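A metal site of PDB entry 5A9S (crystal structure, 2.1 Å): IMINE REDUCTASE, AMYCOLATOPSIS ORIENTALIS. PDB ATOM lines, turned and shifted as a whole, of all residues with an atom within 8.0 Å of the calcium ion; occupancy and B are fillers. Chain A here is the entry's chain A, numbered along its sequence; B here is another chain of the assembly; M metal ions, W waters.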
ATOM      1  N   GLN A 217      -7.975 -24.679 -27.049  1.00  0.00           N
ATOM      2  CA  GLN A 217      -7.250 -24.321 -25.804  1.00  0.00           C
ATOM      3  C   GLN A 217      -7.093 -22.839 -25.644  1.00  0.00           C
ATOM      4  O   GLN A 217      -7.245 -22.306 -24.567  1.00  0.00           O
ATOM      5  CB  GLN A 217      -5.888 -24.982 -25.750  1.00  0.00           C
ATOM      6  CG  GLN A 217      -5.936 -26.485 -25.839  1.00  0.00           C
ATOM      7  CD  GLN A 217      -6.634 -27.025 -24.651  1.00  0.00           C
ATOM      8  OE1 GLN A 217      -7.795 -27.472 -24.742  1.00  0.00           O
ATOM      9  NE2 GLN A 217      -5.971 -26.916 -23.504  1.00  0.00           N
ATOM     10  N   ILE A 218      -6.758 -22.153 -26.704  1.00  0.00           N
ATOM     11  CA  ILE A 218      -6.695 -20.747 -26.582  1.00  0.00           C
ATOM     12  C   ILE A 218      -8.013 -20.020 -26.349  1.00  0.00           C
ATOM     13  O   ILE A 218      -8.017 -19.037 -25.626  1.00  0.00           O
ATOM     14  CB  ILE A 218      -5.797 -19.982 -27.560  1.00  0.00           C
ATOM     15  CG1 ILE A 218      -6.567 -19.147 -28.520  1.00  0.00           C
ATOM     16  CG2 ILE A 218      -4.626 -20.701 -28.248  1.00  0.00           C
ATOM     17  CD1 ILE A 218      -6.002 -17.764 -28.368  1.00  0.00           C
ATOM     18  N   ILE A 219      -9.102 -20.490 -26.948  1.00  0.00           N
ATOM     19  CA  ILE A 219     -10.402 -19.990 -26.600  1.00  0.00           C
ATOM     20  C   ILE A 219     -10.641 -20.173 -25.124  1.00  0.00           C
ATOM     21  O   ILE A 219     -11.037 -19.244 -24.444  1.00  0.00           O
ATOM     22  CB  ILE A 219     -11.523 -20.661 -27.427  1.00  0.00           C
ATOM     23  CG1 ILE A 219     -11.470 -20.131 -28.837  1.00  0.00           C
ATOM     24  CG2 ILE A 219     -12.894 -20.413 -26.784  1.00  0.00           C
ATOM     25  CD1 ILE A 219     -12.323 -20.899 -29.816  1.00  0.00           C
ATOM     26  N   LYS A 220     -10.452 -21.390 -24.633  1.00  0.00           N
ATOM     27  CA  LYS A 220     -10.626 -21.619 -23.173  1.00  0.00           C
ATOM     28  C   LYS A 220      -9.686 -20.791 -22.299  1.00  0.00           C
ATOM     29  O   LYS A 220     -10.117 -20.307 -21.285  1.00  0.00           O
ATOM     30  CB  LYS A 220     -10.457 -23.080 -22.810  1.00  0.00           C
ATOM     31  CG  LYS A 220     -11.621 -23.935 -23.218  1.00  0.00           C
ATOM     32  CD  LYS A 220     -11.210 -25.359 -22.912  1.00  0.00           C
ATOM     33  CE  LYS A 220     -12.314 -26.348 -22.894  1.00  0.00           C
ATOM     34  NZ  LYS A 220     -11.700 -27.707 -22.936  1.00  0.00           N
ATOM     35  N   ALA A 221      -8.423 -20.594 -22.724  1.00  0.00           N
ATOM     36  CA  ALA A 221      -7.491 -19.729 -22.015  1.00  0.00           C
ATOM     37  C   ALA A 221      -8.027 -18.282 -22.047  1.00  0.00           C
ATOM     38  O   ALA A 221      -8.084 -17.623 -21.016  1.00  0.00           O
ATOM     39  CB  ALA A 221      -6.104 -19.768 -22.647  1.00  0.00           C
ATOM     40  N   GLU A 222      -8.457 -17.781 -23.197  1.00  0.00           N
ATOM     41  CA  GLU A 222      -8.937 -16.389 -23.221  1.00  0.00           C
ATOM     42  C   GLU A 222     -10.246 -16.193 -22.424  1.00  0.00           C
ATOM     43  O   GLU A 222     -10.522 -15.096 -21.997  1.00  0.00           O
ATOM     44  CB  GLU A 222      -9.095 -15.915 -24.664  1.00  0.00           C
ATOM     45  CG  GLU A 222      -7.786 -15.626 -25.404  1.00  0.00           C
ATOM     46  CD  GLU A 222      -7.035 -14.397 -24.906  1.00  0.00           C
ATOM     47  OE1 GLU A 222      -7.678 -13.371 -24.431  1.00  0.00           O
ATOM     48  OE2 GLU A 222      -5.782 -14.467 -24.962  1.00  0.00           O
ATOM     49  N   ALA A 223     -11.084 -17.222 -22.316  1.00  0.00           N
ATOM     50  CA  ALA A 223     -12.439 -17.071 -21.727  1.00  0.00           C
ATOM     51  C   ALA A 223     -12.247 -16.707 -20.252  1.00  0.00           C
ATOM     52  O   ALA A 223     -11.633 -17.467 -19.535  1.00  0.00           O
ATOM     53  CB  ALA A 223     -13.256 -18.340 -21.865  1.00  0.00           C
ATOM     54  N   PRO A 224     -12.718 -15.520 -19.831  1.00  0.00           N
ATOM     55  CA  PRO A 224     -12.414 -15.101 -18.478  1.00  0.00           C
ATOM     56  C   PRO A 224     -12.941 -16.065 -17.391  1.00  0.00           C
ATOM     57  O   PRO A 224     -12.407 -16.098 -16.311  1.00  0.00           O
ATOM     58  CB  PRO A 224     -12.999 -13.694 -18.392  1.00  0.00           C
ATOM     59  CG  PRO A 224     -14.003 -13.601 -19.486  1.00  0.00           C
ATOM     60  CD  PRO A 224     -13.490 -14.499 -20.589  1.00  0.00           C
ATOM     61  N   THR A 225     -13.961 -16.868 -17.664  1.00  0.00           N
ATOM     62  CA  THR A 225     -14.512 -17.736 -16.622  1.00  0.00           C
ATOM     63  C   THR A 225     -14.159 -19.173 -16.764  1.00  0.00           C
ATOM     64  O   THR A 225     -14.799 -19.986 -16.163  1.00  0.00           O
ATOM     65  CB  THR A 225     -16.045 -17.605 -16.542  1.00  0.00           C
ATOM     66  OG1 THR A 225     -16.606 -17.919 -17.814  1.00  0.00           O
ATOM     67  CG2 THR A 225     -16.421 -16.198 -16.125  1.00  0.00           C
ATOM     68  N   ILE A 226     -13.130 -19.507 -17.562  1.00  0.00           N
ATOM     69  CA  ILE A 226     -12.607 -20.881 -17.571  1.00  0.00           C
ATOM     70  C   ILE A 226     -11.153 -20.906 -17.164  1.00  0.00           C
ATOM     71  O   ILE A 226     -10.354 -20.095 -17.644  1.00  0.00           O
ATOM     72  CB  ILE A 226     -12.760 -21.506 -18.944  1.00  0.00           C
ATOM     73  CG1 ILE A 226     -14.258 -21.669 -19.213  1.00  0.00           C
ATOM     74  CG2 ILE A 226     -12.028 -22.837 -19.005  1.00  0.00           C
ATOM     75  CD1 ILE A 226     -14.575 -22.215 -20.561  1.00  0.00           C
ATOM     76  N   ASP A 227     -10.810 -21.784 -16.247  1.00  0.00           N
ATOM     77  CA  ASP A 227      -9.427 -22.027 -15.890  1.00  0.00           C
ATOM     78  C   ASP A 227      -9.250 -23.531 -15.642  1.00  0.00           C
ATOM     79  O   ASP A 227      -8.922 -24.271 -16.564  1.00  0.00           O
ATOM     80  CB  ASP A 227      -9.078 -21.282 -14.664  1.00  0.00           C
ATOM     81  CG  ASP A 227      -7.766 -21.709 -14.122  1.00  0.00           C
ATOM     82  OD1 ASP A 227      -7.732 -22.795 -13.503  1.00  0.00           O
ATOM     83  OD2 ASP A 227      -6.768 -20.996 -14.342  1.00  0.00           O
ATOM     84  N   ASP A 234      -1.907 -17.890 -22.992  1.00  0.00           N
ATOM     85  CA  ASP A 234      -3.030 -17.261 -23.719  1.00  0.00           C
ATOM     86  C   ASP A 234      -2.577 -16.635 -25.052  1.00  0.00           C
ATOM     87  O   ASP A 234      -1.436 -16.826 -25.455  1.00  0.00           O
ATOM     88  CB  ASP A 234      -3.810 -16.239 -22.802  1.00  0.00           C
ATOM     89  CG  ASP A 234      -2.992 -15.005 -22.405  1.00  0.00           C
ATOM     90  OD1 ASP A 234      -2.339 -14.382 -23.261  1.00  0.00           O
ATOM     91  OD2 ASP A 234      -3.005 -14.641 -21.220  1.00  0.00           O
ATOM     92  N   TYR A 283      -9.673 -11.323 -25.760  1.00  0.00           N
ATOM     93  CA  TYR A 283     -11.104 -11.565 -25.524  1.00  0.00           C
ATOM     94  C   TYR A 283     -11.866 -10.284 -25.524  1.00  0.00           C
ATOM     95  O   TYR A 283     -13.033 -10.262 -25.947  1.00  0.00           O
ATOM     96  CB  TYR A 283     -11.354 -12.300 -24.205  1.00  0.00           C
ATOM     97  CG  TYR A 283     -12.698 -12.979 -24.113  1.00  0.00           C
ATOM     98  CD1 TYR A 283     -13.824 -12.300 -23.630  1.00  0.00           C
ATOM     99  CD2 TYR A 283     -12.836 -14.317 -24.468  1.00  0.00           C
ATOM    100  CE1 TYR A 283     -15.055 -12.918 -23.538  1.00  0.00           C
ATOM    101  CE2 TYR A 283     -14.057 -14.954 -24.356  1.00  0.00           C
ATOM    102  CZ  TYR A 283     -15.155 -14.239 -23.897  1.00  0.00           C
ATOM    103  OH  TYR A 283     -16.345 -14.854 -23.854  1.00  0.00           O
ATOM    104  N   THR B 203     -19.072 -22.088 -23.481  1.00  0.00           N
ATOM    105  CA  THR B 203     -17.707 -22.183 -24.039  1.00  0.00           C
ATOM    106  C   THR B 203     -17.296 -23.647 -24.089  1.00  0.00           C
ATOM    107  O   THR B 203     -16.707 -24.077 -25.074  1.00  0.00           O
ATOM    108  CB  THR B 203     -16.690 -21.333 -23.241  1.00  0.00           C
ATOM    109  OG1 THR B 203     -17.063 -19.933 -23.326  1.00  0.00           O
ATOM    110  CG2 THR B 203     -15.271 -21.497 -23.788  1.00  0.00           C
HETATM  111 CA    CA M   1      -9.701 -18.739 -19.433  1.00  0.00          CA
HETATM  112  O   HOH W   1      -8.583 -17.044 -17.861  1.00  0.00           O
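Glu 222 touches the calcium ion.
Along chain A the residues within 4 Å of the calcium ion span positions 220 to 226.
The nearest printed residue that does not touch the calcium ion is Pro 224 (4.4 Å).
The side-chain carboxylate (OE1) of Glu 222 lies within hydrogen-bond range of the backbone NH (N) of Tyr 283 (3.2 Å).
O of Ala 223 binds the calcium ion (2.3 Å).
O of Ile 226 binds the calcium ion (2.3 Å).
O of Lys 220 is bound to the calcium ion (2.5 Å).
O of Ala 221 binds the calcium ion, at 2.5 Å.
Water W1 binds the calcium ion (2.6 Å).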
